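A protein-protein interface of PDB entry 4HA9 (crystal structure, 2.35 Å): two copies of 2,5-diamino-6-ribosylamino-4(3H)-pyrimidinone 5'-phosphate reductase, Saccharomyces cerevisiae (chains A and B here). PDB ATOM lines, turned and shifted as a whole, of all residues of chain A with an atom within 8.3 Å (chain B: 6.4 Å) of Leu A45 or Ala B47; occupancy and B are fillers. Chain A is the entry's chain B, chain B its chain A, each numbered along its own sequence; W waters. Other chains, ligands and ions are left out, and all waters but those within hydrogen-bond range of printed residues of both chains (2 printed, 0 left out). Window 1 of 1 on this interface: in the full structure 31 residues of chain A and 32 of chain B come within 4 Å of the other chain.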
ATOM      1  N   ALA A  42      12.612  22.178   9.729  1.00  0.00           N
ATOM      2  CA  ALA A  42      11.964  20.922  10.061  1.00  0.00           C
ATOM      3  C   ALA A  42      13.041  19.846  10.088  1.00  0.00           C
ATOM      4  O   ALA A  42      13.799  19.699   9.123  1.00  0.00           O
ATOM      5  CB  ALA A  42      10.911  20.576   9.008  1.00  0.00           C
ATOM      6  N   GLN A  43      13.123  19.113  11.198  1.00  0.00           N
ATOM      7  CA  GLN A  43      14.151  18.088  11.365  1.00  0.00           C
ATOM      8  C   GLN A  43      13.552  16.784  11.854  1.00  0.00           C
ATOM      9  O   GLN A  43      12.421  16.751  12.330  1.00  0.00           O
ATOM     10  CB  GLN A  43      15.235  18.539  12.346  1.00  0.00           C
ATOM     11  CG  GLN A  43      14.735  18.806  13.750  1.00  0.00           C
ATOM     12  CD  GLN A  43      15.865  18.967  14.745  1.00  0.00           C
ATOM     13  OE1 GLN A  43      16.930  19.459  14.404  1.00  0.00           O
ATOM     14  NE2 GLN A  43      15.647  18.519  15.979  1.00  0.00           N
ATOM     15  N   SER A  44      14.327  15.715  11.714  1.00  0.00           N
ATOM     16  CA  SER A  44      13.983  14.414  12.244  1.00  0.00           C
ATOM     17  C   SER A  44      14.457  14.390  13.684  1.00  0.00           C
ATOM     18  O   SER A  44      15.032  15.365  14.157  1.00  0.00           O
ATOM     19  CB  SER A  44      14.736  13.341  11.469  1.00  0.00           C
ATOM     20  OG  SER A  44      16.116  13.689  11.384  1.00  0.00           O
ATOM     21  N   LEU A  45      14.248  13.272  14.371  1.00  0.00           N
ATOM     22  CA  LEU A  45      14.678  13.152  15.760  1.00  0.00           C
ATOM     23  C   LEU A  45      16.183  13.254  15.838  1.00  0.00           C
ATOM     24  O   LEU A  45      16.710  13.866  16.759  1.00  0.00           O
ATOM     25  CB  LEU A  45      14.226  11.826  16.356  1.00  0.00           C
ATOM     26  CG  LEU A  45      12.721  11.714  16.556  1.00  0.00           C
ATOM     27  CD1 LEU A  45      12.326  10.250  16.673  1.00  0.00           C
ATOM     28  CD2 LEU A  45      12.327  12.491  17.791  1.00  0.00           C
ATOM     29  N   ASP A  46      16.874  12.672  14.857  1.00  0.00           N
ATOM     30  CA  ASP A  46      18.328  12.771  14.836  1.00  0.00           C
ATOM     31  C   ASP A  46      18.861  14.083  14.221  1.00  0.00           C
ATOM     32  O   ASP A  46      19.986  14.123  13.724  1.00  0.00           O
ATOM     33  CB  ASP A  46      19.013  11.511  14.263  1.00  0.00           C
ATOM     34  CG  ASP A  46      18.460  11.066  12.921  1.00  0.00           C
ATOM     35  OD1 ASP A  46      17.410  11.570  12.471  1.00  0.00           O
ATOM     36  OD2 ASP A  46      19.084  10.164  12.317  1.00  0.00           O
ATOM     37  N   ALA A  47      18.057  15.151  14.285  1.00  0.00           N
ATOM     38  CA  ALA A  47      18.519  16.497  13.904  1.00  0.00           C
ATOM     39  C   ALA A  47      18.946  16.634  12.432  1.00  0.00           C
ATOM     40  O   ALA A  47      19.872  17.379  12.113  1.00  0.00           O
ATOM     41  CB  ALA A  47      19.667  16.941  14.823  1.00  0.00           C
ATOM     42  N   ARG A  48      18.280  15.919  11.537  1.00  0.00           N
ATOM     43  CA  ARG A  48      18.635  15.998  10.136  1.00  0.00           C
ATOM     44  C   ARG A  48      17.561  16.708   9.296  1.00  0.00           C
ATOM     45  O   ARG A  48      16.364  16.619   9.573  1.00  0.00           O
ATOM     46  CB  ARG A  48      19.004  14.612   9.591  1.00  0.00           C
ATOM     47  CG  ARG A  48      20.515  14.399   9.538  1.00  0.00           C
ATOM     48  CD  ARG A  48      20.991  13.197  10.322  1.00  0.00           C
ATOM     49  NE  ARG A  48      21.525  13.544  11.637  1.00  0.00           N
ATOM     50  CZ  ARG A  48      22.809  13.497  11.988  1.00  0.00           C
ATOM     51  NH1 ARG A  48      23.755  13.124  11.129  1.00  0.00           N
ATOM     52  NH2 ARG A  48      23.148  13.834  13.225  1.00  0.00           N
ATOM     53  N   VAL A  49      17.996  17.464   8.298  1.00  0.00           N
ATOM     54  CA  VAL A  49      17.043  18.200   7.500  1.00  0.00           C
ATOM     55  C   VAL A  49      16.923  17.569   6.124  1.00  0.00           C
ATOM     56  O   VAL A  49      16.119  18.006   5.316  1.00  0.00           O
ATOM     57  CB  VAL A  49      17.384  19.710   7.396  1.00  0.00           C
ATOM     58  CG1 VAL A  49      17.316  20.346   8.747  1.00  0.00           C
ATOM     59  CG2 VAL A  49      18.757  19.933   6.773  1.00  0.00           C
ATOM     60  N   THR A 207      10.402  22.408  13.852  1.00  0.00           N
ATOM     61  CA  THR A 207       9.474  21.294  13.822  1.00  0.00           C
ATOM     62  C   THR A 207      10.325  20.037  13.958  1.00  0.00           C
ATOM     63  O   THR A 207      11.379  19.930  13.321  1.00  0.00           O
ATOM     64  CB  THR A 207       8.690  21.277  12.499  1.00  0.00           C
ATOM     65  OG1 THR A 207       7.901  22.465  12.394  1.00  0.00           O
ATOM     66  CG2 THR A 207       7.772  20.045  12.387  1.00  0.00           C
ATOM     67  N   ILE A 208       9.908  19.109  14.813  1.00  0.00           N
ATOM     68  CA  ILE A 208      10.613  17.829  14.913  1.00  0.00           C
ATOM     69  C   ILE A 208       9.675  16.689  14.528  1.00  0.00           C
ATOM     70  O   ILE A 208       8.601  16.525  15.107  1.00  0.00           O
ATOM     71  CB  ILE A 208      11.200  17.569  16.321  1.00  0.00           C
ATOM     72  CG1 ILE A 208      11.934  18.798  16.855  1.00  0.00           C
ATOM     73  CG2 ILE A 208      12.157  16.383  16.288  1.00  0.00           C
ATOM     74  CD1 ILE A 208      12.565  18.550  18.210  1.00  0.00           C
ATOM     75  N   GLY A 209      10.070  15.920  13.527  1.00  0.00           N
ATOM     76  CA  GLY A 209       9.249  14.825  13.051  1.00  0.00           C
ATOM     77  C   GLY A 209       9.628  13.551  13.774  1.00  0.00           C
ATOM     78  O   GLY A 209      10.802  13.341  14.073  1.00  0.00           O
ATOM     79  N   SER A 210       8.639  12.707  14.058  1.00  0.00           N
ATOM     80  CA  SER A 210       8.879  11.468  14.787  1.00  0.00           C
ATOM     81  C   SER A 210       9.466  10.383  13.901  1.00  0.00           C
ATOM     82  O   SER A 210       8.861   9.328  13.720  1.00  0.00           O
ATOM     83  CB  SER A 210       7.611  10.966  15.478  1.00  0.00           C
ATOM     84  OG  SER A 210       6.533  10.868  14.576  1.00  0.00           O
ATOM     85  N   THR A 211      10.652  10.655  13.358  1.00  0.00           N
ATOM     86  CA  THR A 211      11.345   9.692  12.522  1.00  0.00           C
ATOM     87  C   THR A 211      12.850   9.888  12.590  1.00  0.00           C
ATOM     88  O   THR A 211      13.317  10.896  13.075  1.00  0.00           O
ATOM     89  CB  THR A 211      10.842   9.736  11.053  1.00  0.00           C
ATOM     90  OG1 THR A 211      11.313   8.583  10.362  1.00  0.00           O
ATOM     91  CG2 THR A 211      11.321  10.978  10.317  1.00  0.00           C
ATOM     92  N   PHE A 212      13.609   8.912  12.110  1.00  0.00           N
ATOM     93  CA  PHE A 212      15.056   9.035  12.052  1.00  0.00           C
ATOM     94  C   PHE A 212      15.431   9.010  10.579  1.00  0.00           C
ATOM     95  O   PHE A 212      15.021   8.118   9.865  1.00  0.00           O
ATOM     96  CB  PHE A 212      15.735   7.860  12.762  1.00  0.00           C
ATOM     97  CG  PHE A 212      15.627   7.896  14.264  1.00  0.00           C
ATOM     98  CD1 PHE A 212      16.522   8.639  15.026  1.00  0.00           C
ATOM     99  CD2 PHE A 212      14.649   7.164  14.921  1.00  0.00           C
ATOM    100  CE1 PHE A 212      16.442   8.649  16.409  1.00  0.00           C
ATOM    101  CE2 PHE A 212      14.564   7.184  16.312  1.00  0.00           C
ATOM    102  CZ  PHE A 212      15.461   7.935  17.050  1.00  0.00           C
ATOM    103  N   LEU A 213      16.207   9.986  10.126  1.00  0.00           N
ATOM    104  CA  LEU A 213      16.601  10.046   8.721  1.00  0.00           C
ATOM    105  C   LEU A 213      17.893   9.300   8.428  1.00  0.00           C
ATOM    106  O   LEU A 213      18.158   8.953   7.282  1.00  0.00           O
ATOM    107  CB  LEU A 213      16.726  11.490   8.238  1.00  0.00           C
ATOM    108  CG  LEU A 213      15.399  12.181   7.928  1.00  0.00           C
ATOM    109  CD1 LEU A 213      15.644  13.471   7.175  1.00  0.00           C
ATOM    110  CD2 LEU A 213      14.481  11.261   7.139  1.00  0.00           C
ATOM    111  N   GLY A 214      18.696   9.044   9.457  1.00  0.00           N
ATOM    112  CA  GLY A 214      19.934   8.303   9.267  1.00  0.00           C
ATOM    113  C   GLY A 214      21.139   9.216   9.364  1.00  0.00           C
ATOM    114  O   GLY A 214      21.037  10.419   9.082  1.00  0.00           O
ATOM    115  N   GLU A 219      23.007  17.378   8.883  1.00  0.00           N
ATOM    116  CA  GLU A 219      22.571  17.746  10.217  1.00  0.00           C
ATOM    117  C   GLU A 219      22.540  19.256  10.425  1.00  0.00           C
ATOM    118  O   GLU A 219      23.295  20.006   9.813  1.00  0.00           O
ATOM    119  CB  GLU A 219      23.457  17.092  11.286  1.00  0.00           C
ATOM    120  CG  GLU A 219      24.738  17.856  11.599  1.00  0.00           C
ATOM    121  CD  GLU A 219      25.466  17.355  12.854  1.00  0.00           C
ATOM    122  OE1 GLU A 219      26.568  17.875  13.144  1.00  0.00           O
ATOM    123  OE2 GLU A 219      24.944  16.456  13.547  1.00  0.00           O
ATOM    124  N   VAL A 220      21.648  19.687  11.303  1.00  0.00           N
ATOM    125  CA  VAL A 220      21.762  20.999  11.899  1.00  0.00           C
ATOM    126  C   VAL A 220      22.280  20.834  13.329  1.00  0.00           C
ATOM    127  O   VAL A 220      21.615  20.244  14.191  1.00  0.00           O
ATOM    128  CB  VAL A 220      20.422  21.723  11.878  1.00  0.00           C
ATOM    129  CG1 VAL A 220      19.323  20.716  12.116  1.00  0.00           C
ATOM    130  CG2 VAL A 220      20.403  22.837  12.917  1.00  0.00           C
ATOM    131  N   SER A 221      23.489  21.329  13.566  1.00  0.00           N
ATOM    132  CA  SER A 221      24.067  21.313  14.898  1.00  0.00           C
ATOM    133  C   SER A 221      25.158  22.352  14.946  1.00  0.00           C
ATOM    134  O   SER A 221      26.184  22.193  14.298  1.00  0.00           O
ATOM    135  CB  SER A 221      24.664  19.942  15.226  1.00  0.00           C
ATOM    136  OG  SER A 221      25.279  19.947  16.510  1.00  0.00           O
ATOM    137  N   THR A 238       2.095  13.501  14.964  1.00  0.00           N
ATOM    138  CA  THR A 238       3.364  12.910  14.573  1.00  0.00           C
ATOM    139  C   THR A 238       4.495  13.888  14.831  1.00  0.00           C
ATOM    140  O   THR A 238       5.657  13.507  14.830  1.00  0.00           O
ATOM    141  CB  THR A 238       3.387  12.579  13.063  1.00  0.00           C
ATOM    142  OG1 THR A 238       3.074  13.760  12.306  1.00  0.00           O
ATOM    143  CG2 THR A 238       2.382  11.494  12.731  1.00  0.00           C
ATOM    144  N   VAL A 240       6.151  17.647  16.727  1.00  0.00           N
ATOM    145  CA  VAL A 240       6.160  18.561  17.838  1.00  0.00           C
ATOM    146  C   VAL A 240       6.788  19.846  17.281  1.00  0.00           C
ATOM    147  O   VAL A 240       7.652  19.787  16.403  1.00  0.00           O
ATOM    148  CB  VAL A 240       6.937  17.901  19.024  1.00  0.00           C
ATOM    149  CG1 VAL A 240       8.404  18.277  19.027  1.00  0.00           C
ATOM    150  CG2 VAL A 240       6.266  18.172  20.340  1.00  0.00           C
ATOM    151  N   TYR B  41      16.457   7.391  26.306  1.00  0.00           N
ATOM    152  CA  TYR B  41      17.579   8.322  26.410  1.00  0.00           C
ATOM    153  C   TYR B  41      17.127   9.786  26.307  1.00  0.00           C
ATOM    154  O   TYR B  41      16.020  10.073  25.863  1.00  0.00           O
ATOM    155  CB  TYR B  41      18.658   8.001  25.370  1.00  0.00           C
ATOM    156  CG  TYR B  41      18.252   8.212  23.915  1.00  0.00           C
ATOM    157  CD1 TYR B  41      18.425   9.447  23.299  1.00  0.00           C
ATOM    158  CD2 TYR B  41      17.722   7.174  23.153  1.00  0.00           C
ATOM    159  CE1 TYR B  41      18.071   9.651  21.971  1.00  0.00           C
ATOM    160  CE2 TYR B  41      17.372   7.368  21.812  1.00  0.00           C
ATOM    161  CZ  TYR B  41      17.544   8.610  21.240  1.00  0.00           C
ATOM    162  OH  TYR B  41      17.201   8.826  19.937  1.00  0.00           O
ATOM    163  N   GLN B  43      18.140  13.592  24.944  1.00  0.00           N
ATOM    164  CA  GLN B  43      19.016  14.298  24.000  1.00  0.00           C
ATOM    165  C   GLN B  43      18.740  15.789  23.923  1.00  0.00           C
ATOM    166  O   GLN B  43      17.692  16.272  24.343  1.00  0.00           O
ATOM    167  CB  GLN B  43      18.921  13.695  22.598  1.00  0.00           C
ATOM    168  CG  GLN B  43      17.557  13.862  21.970  1.00  0.00           C
ATOM    169  CD  GLN B  43      17.483  13.359  20.538  1.00  0.00           C
ATOM    170  OE1 GLN B  43      18.148  12.402  20.157  1.00  0.00           O
ATOM    171  NE2 GLN B  43      16.660  14.007  19.742  1.00  0.00           N
ATOM    172  N   SER B  44      19.718  16.516  23.411  1.00  0.00           N
ATOM    173  CA  SER B  44      19.554  17.918  23.040  1.00  0.00           C
ATOM    174  C   SER B  44      18.701  18.002  21.768  1.00  0.00           C
ATOM    175  O   SER B  44      18.389  16.977  21.163  1.00  0.00           O
ATOM    176  CB  SER B  44      20.928  18.505  22.750  1.00  0.00           C
ATOM    177  OG  SER B  44      21.608  17.669  21.809  1.00  0.00           O
ATOM    178  N   LEU B  45      18.364  19.217  21.336  1.00  0.00           N
ATOM    179  CA  LEU B  45      17.683  19.394  20.043  1.00  0.00           C
ATOM    180  C   LEU B  45      18.504  18.876  18.873  1.00  0.00           C
ATOM    181  O   LEU B  45      17.950  18.321  17.924  1.00  0.00           O
ATOM    182  CB  LEU B  45      17.364  20.855  19.791  1.00  0.00           C
ATOM    183  CG  LEU B  45      16.274  21.462  20.650  1.00  0.00           C
ATOM    184  CD1 LEU B  45      16.390  22.933  20.520  1.00  0.00           C
ATOM    185  CD2 LEU B  45      14.926  20.989  20.176  1.00  0.00           C
ATOM    186  N   ASP B  46      19.824  19.050  18.944  1.00  0.00           N
ATOM    187  CA  ASP B  46      20.712  18.510  17.903  1.00  0.00           C
ATOM    188  C   ASP B  46      21.094  17.035  18.095  1.00  0.00           C
ATOM    189  O   ASP B  46      22.150  16.577  17.657  1.00  0.00           O
ATOM    190  CB  ASP B  46      21.935  19.422  17.611  1.00  0.00           C
ATOM    191  CG  ASP B  46      22.721  19.843  18.863  1.00  0.00           C
ATOM    192  OD1 ASP B  46      22.182  19.779  19.983  1.00  0.00           O
ATOM    193  OD2 ASP B  46      23.907  20.266  18.706  1.00  0.00           O
ATOM    194  N   ALA B  47      20.205  16.297  18.744  1.00  0.00           N
ATOM    195  CA  ALA B  47      20.355  14.849  18.935  1.00  0.00           C
ATOM    196  C   ALA B  47      21.656  14.439  19.600  1.00  0.00           C
ATOM    197  O   ALA B  47      22.260  13.442  19.239  1.00  0.00           O
ATOM    198  CB  ALA B  47      20.166  14.103  17.634  1.00  0.00           C
ATOM    199  N   ARG B  48      22.087  15.221  20.575  1.00  0.00           N
ATOM    200  CA  ARG B  48      23.284  14.874  21.293  1.00  0.00           C
ATOM    201  C   ARG B  48      22.909  14.427  22.698  1.00  0.00           C
ATOM    202  O   ARG B  48      21.969  14.960  23.297  1.00  0.00           O
ATOM    203  CB  ARG B  48      24.271  16.038  21.277  1.00  0.00           C
ATOM    204  CG  ARG B  48      25.569  15.660  20.618  1.00  0.00           C
ATOM    205  CD  ARG B  48      25.920  16.458  19.373  1.00  0.00           C
ATOM    206  NE  ARG B  48      25.012  16.220  18.268  1.00  0.00           N
ATOM    207  CZ  ARG B  48      25.359  16.176  16.985  1.00  0.00           C
ATOM    208  NH1 ARG B  48      26.628  16.324  16.605  1.00  0.00           N
ATOM    209  NH2 ARG B  48      24.416  15.966  16.075  1.00  0.00           N
ATOM    210  N   VAL B  49      23.585  13.390  23.189  1.00  0.00           N
ATOM    211  CA  VAL B  49      23.366  12.908  24.559  1.00  0.00           C
ATOM    212  C   VAL B  49      24.486  13.416  25.470  1.00  0.00           C
ATOM    213  O   VAL B  49      24.370  13.388  26.694  1.00  0.00           O
ATOM    214  CB  VAL B  49      23.258  11.345  24.649  1.00  0.00           C
ATOM    215  CG1 VAL B  49      22.018  10.830  23.919  1.00  0.00           C
ATOM    216  CG2 VAL B  49      24.495  10.672  24.100  1.00  0.00           C
ATOM    217  N   LEU B 204      10.391   2.658  22.614  1.00  0.00           N
ATOM    218  CA  LEU B 204      11.362   3.726  22.461  1.00  0.00           C
ATOM    219  C   LEU B 204      10.784   4.956  23.141  1.00  0.00           C
ATOM    220  O   LEU B 204       9.662   5.370  22.870  1.00  0.00           O
ATOM    221  CB  LEU B 204      11.636   4.000  20.981  1.00  0.00           C
ATOM    222  CG  LEU B 204      12.545   5.190  20.643  1.00  0.00           C
ATOM    223  CD1 LEU B 204      13.986   5.022  21.181  1.00  0.00           C
ATOM    224  CD2 LEU B 204      12.556   5.408  19.133  1.00  0.00           C
ATOM    225  N   ILE B 206      12.021   8.793  24.239  1.00  0.00           N
ATOM    226  CA  ILE B 206      13.092   9.764  24.089  1.00  0.00           C
ATOM    227  C   ILE B 206      12.686  11.079  24.718  1.00  0.00           C
ATOM    228  O   ILE B 206      11.579  11.546  24.477  1.00  0.00           O
ATOM    229  CB  ILE B 206      13.348  10.027  22.610  1.00  0.00           C
ATOM    230  CG1 ILE B 206      13.617   8.717  21.875  1.00  0.00           C
ATOM    231  CG2 ILE B 206      14.486  11.023  22.425  1.00  0.00           C
ATOM    232  CD1 ILE B 206      13.672   8.890  20.365  1.00  0.00           C
ATOM    233  N   ILE B 208      13.483  15.036  24.713  1.00  0.00           N
ATOM    234  CA  ILE B 208      14.170  16.088  23.953  1.00  0.00           C
ATOM    235  C   ILE B 208      14.121  17.387  24.732  1.00  0.00           C
ATOM    236  O   ILE B 208      13.049  17.920  24.984  1.00  0.00           O
ATOM    237  CB  ILE B 208      13.546  16.321  22.561  1.00  0.00           C
ATOM    238  CG1 ILE B 208      13.469  15.005  21.801  1.00  0.00           C
ATOM    239  CG2 ILE B 208      14.378  17.344  21.770  1.00  0.00           C
ATOM    240  CD1 ILE B 208      12.846  15.139  20.434  1.00  0.00           C
ATOM    241  N   THR B 218      28.531  13.907  21.707  1.00  0.00           N
ATOM    242  CA  THR B 218      28.282  12.607  21.078  1.00  0.00           C
ATOM    243  C   THR B 218      26.817  12.419  20.708  1.00  0.00           C
ATOM    244  O   THR B 218      25.925  12.575  21.533  1.00  0.00           O
ATOM    245  CB  THR B 218      28.893  11.383  21.847  1.00  0.00           C
ATOM    246  OG1 THR B 218      27.865  10.548  22.377  1.00  0.00           O
ATOM    247  CG2 THR B 218      29.853  11.820  22.954  1.00  0.00           C
ATOM    248  N   GLU B 219      26.590  12.094  19.440  1.00  0.00           N
ATOM    249  CA  GLU B 219      25.253  12.077  18.872  1.00  0.00           C
ATOM    250  C   GLU B 219      24.631  10.686  18.825  1.00  0.00           C
ATOM    251  O   GLU B 219      25.327   9.664  18.756  1.00  0.00           O
ATOM    252  CB  GLU B 219      25.262  12.682  17.455  1.00  0.00           C
ATOM    253  CG  GLU B 219      25.428  11.676  16.332  1.00  0.00           C
ATOM    254  CD  GLU B 219      25.390  12.305  14.945  1.00  0.00           C
ATOM    255  OE1 GLU B 219      25.381  11.556  13.947  1.00  0.00           O
ATOM    256  OE2 GLU B 219      25.373  13.547  14.843  1.00  0.00           O
ATOM    257  N   VAL B 220      23.304  10.668  18.851  1.00  0.00           N
ATOM    258  CA  VAL B 220      22.558   9.468  18.561  1.00  0.00           C
ATOM    259  C   VAL B 220      21.817   9.627  17.232  1.00  0.00           C
ATOM    260  O   VAL B 220      20.889  10.430  17.083  1.00  0.00           O
ATOM    261  CB  VAL B 220      21.620   9.075  19.722  1.00  0.00           C
ATOM    262  CG1 VAL B 220      21.069  10.299  20.342  1.00  0.00           C
ATOM    263  CG2 VAL B 220      20.516   8.159  19.218  1.00  0.00           C
ATOM    264  N   SER B 221      22.276   8.857  16.259  1.00  0.00           N
ATOM    265  CA  SER B 221      21.704   8.836  14.940  1.00  0.00           C
ATOM    266  C   SER B 221      22.086   7.491  14.339  1.00  0.00           C
ATOM    267  O   SER B 221      23.262   7.149  14.265  1.00  0.00           O
ATOM    268  CB  SER B 221      22.271   9.987  14.106  1.00  0.00           C
ATOM    269  OG  SER B 221      21.685  10.031  12.813  1.00  0.00           O
ATOM    270  N   LEU B 228       9.108   4.897  12.705  1.00  0.00           N
ATOM    271  CA  LEU B 228       8.458   4.600  13.974  1.00  0.00           C
ATOM    272  C   LEU B 228       6.956   4.355  13.774  1.00  0.00           C
ATOM    273  O   LEU B 228       6.410   4.635  12.702  1.00  0.00           O
ATOM    274  CB  LEU B 228       8.664   5.769  14.939  1.00  0.00           C
ATOM    275  CG  LEU B 228       9.919   5.854  15.819  1.00  0.00           C
ATOM    276  CD1 LEU B 228      11.110   5.127  15.240  1.00  0.00           C
ATOM    277  CD2 LEU B 228      10.276   7.315  16.113  1.00  0.00           C
ATOM    278  N   TRP B 233       3.283  11.852  21.991  1.00  0.00           N
ATOM    279  CA  TRP B 233       4.149  12.877  22.527  1.00  0.00           C
ATOM    280  C   TRP B 233       3.591  13.405  23.818  1.00  0.00           C
ATOM    281  O   TRP B 233       2.383  13.447  24.000  1.00  0.00           O
ATOM    282  CB  TRP B 233       4.216  14.047  21.562  1.00  0.00           C
ATOM    283  CG  TRP B 233       5.053  13.835  20.359  1.00  0.00           C
ATOM    284  CD1 TRP B 233       4.621  13.532  19.097  1.00  0.00           C
ATOM    285  CD2 TRP B 233       6.473  13.961  20.279  1.00  0.00           C
ATOM    286  NE1 TRP B 233       5.684  13.457  18.241  1.00  0.00           N
ATOM    287  CE2 TRP B 233       6.835  13.715  18.943  1.00  0.00           C
ATOM    288  CE3 TRP B 233       7.474  14.244  21.212  1.00  0.00           C
ATOM    289  CZ2 TRP B 233       8.153  13.748  18.515  1.00  0.00           C
ATOM    290  CZ3 TRP B 233       8.775  14.289  20.785  1.00  0.00           C
ATOM    291  CH2 TRP B 233       9.107  14.039  19.450  1.00  0.00           C
ATOM    292  N   LEU B 242       8.897  11.640  23.626  1.00  0.00           N
ATOM    293  CA  LEU B 242       8.281  10.774  22.618  1.00  0.00           C
ATOM    294  C   LEU B 242       8.229   9.338  23.139  1.00  0.00           C
ATOM    295  O   LEU B 242       9.253   8.787  23.499  1.00  0.00           O
ATOM    296  CB  LEU B 242       9.157  10.755  21.355  1.00  0.00           C
ATOM    297  CG  LEU B 242       8.626  10.366  19.960  1.00  0.00           C
ATOM    298  CD1 LEU B 242       9.587   9.482  19.199  1.00  0.00           C
ATOM    299  CD2 LEU B 242       7.281   9.742  19.976  1.00  0.00           C
HETATM  300  O   HOH W   1       8.779   7.353  11.496  1.00  0.00           O
HETATM  301  O   HOH W   2      15.732  16.389  18.093  1.00  0.00           O
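The side-chain carboxylate of Glu B219 lies within salt-bridge range of the guanidinium group of Arg A48 (2.8 Å).
The guanidinium group (NH2) of Arg B48 is in salt-bridge range of the side-chain carboxylate (OE2) of Glu A219.
The indole nitrogen of Trp B233 lies within hydrogen-bond range of the backbone carbonyl oxygen of Thr A238, at 3.4 Å.
The backbone carbonyl oxygen (O) of Leu B45 is in hydrogen-bond range of the side-chain amide nitrogen (NE2) of Gln A43, 3.0 Å away.
The side-chain carboxylate (OE2) of Glu A219 lies close to the side-chain carboxylate (OE2) of Glu B219 (3.2 Å).
OD2 of Asp A46 is in hydrogen-bond range of OG of Ser B221.
NE2 of Gln B43 is in hydrogen-bond range of O of Leu A45 (3.0 Å).
The side-chain carboxylate (OD2) of Asp B46 sits at hydrogen-bond distance from the side-chain hydroxyl (OG) of Ser A221, 2.6 Å away.
N of Ile A208 sits at hydrogen-bond distance from O of Val A240 (2.8 Å).
The backbone NH of Arg A48 sits at hydrogen-bond distance from the side-chain hydroxyl of Ser A44, 3.1 Å away.
N of Val A220 is in hydrogen-bond range of O of Ala A47 (3.0 Å).
OD2 of Asp A46 is in hydrogen-bond range of N of Gly A214.
The side-chain carboxylate (OD1) of Asp B46 lies within hydrogen-bond range of the side-chain hydroxyl (OG) of Ser B44, at 2.8 Å.
The backbone carbonyl oxygen of Thr A211 is in hydrogen-bond range of the backbone NH of Leu A45.
Among the printed residues, merely in contact across the chains: Leu A45 with Ala B47, Leu A45 with Ile B208, Leu A45 with Leu B228, Leu A45 with Trp B233, Leu A45 with Leu B242, Asp A46 with Ala B47, Asp A46 with Val B220, Ala A47 with Leu B45, Ala A47 with Asp B46, Arg A48 with Arg B48, Arg A48 with Ser B221, Ile A208 with Leu B45, Ser A210 with Leu B228, Phe A212 with Tyr B41, Phe A212 with Leu B204, Phe A212 with Ile B206, Gly A214 with Ser B221, Val A220 with Asp B46 and Ser A221 with Arg B48.
Of the printed residues of chain B, Leu A45 touches Gln B43, Ala B47, Ile B208, Leu B228, Trp B233 and Leu B242.
Printed residues of chain B within 4 Å of Arg A48: Arg B48 (3.8 Å), Glu B219 (2.8 Å) and Ser B221 (3.7 Å).
Of the printed residues of chain B, Ile A208 touches Leu B45 (3.9 Å).
Ser B44 touches none of the printed residues of chain A.
Printed residues of chain A within 4 Å of Leu B45: Gln A43, Ala A47 and Ile A208.
Printed residues of chain A within 4 Å of Ala B47: Leu A45 (3.6 Å) and Asp A46 (3.6 Å).
The nearest residue of chain B that does not touch Leu A45 is Ile B206 (4.2 Å).
The nearest printed residue of chain A that does not touch Ala B47 is Ala A47 (4.01 Å).
The nearest printed residue of chain A that does not touch Trp B233 is Ser A210 (4.2 Å).
Of the 21 printed residues of chain A, 13 touch a printed residue of chain B.
Among the printed residues, 27 pairs touch across the chains.
Asp A46 touches Ala B47, and with the chains exchanged Ala A47 touches Asp B46.
Asp A46 touches Ser B221, and with the chains exchanged Ser A221 touches Asp B46.
Arg B48 touches its own counterpart, Arg A48.
Arg A48 touches Glu B219, and with the chains exchanged Glu A219 touches Arg B48.
11 positions are printed for both chains.
Water W1 lies within hydrogen-bond range of the backbone NH of Leu B228, the backbone carbonyl oxygen of Ser A210 and the side-chain hydroxyl of Thr A211.
Water W2 lies within hydrogen-bond range of the backbone carbonyl oxygen of Leu B45 (2.9 Å), the side-chain amide nitrogen of Gln A43 (3.0 Å), the backbone carbonyl oxygen of Leu A45 (3.0 Å) and the side-chain amide nitrogen of Gln B43 (3.0 Å).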
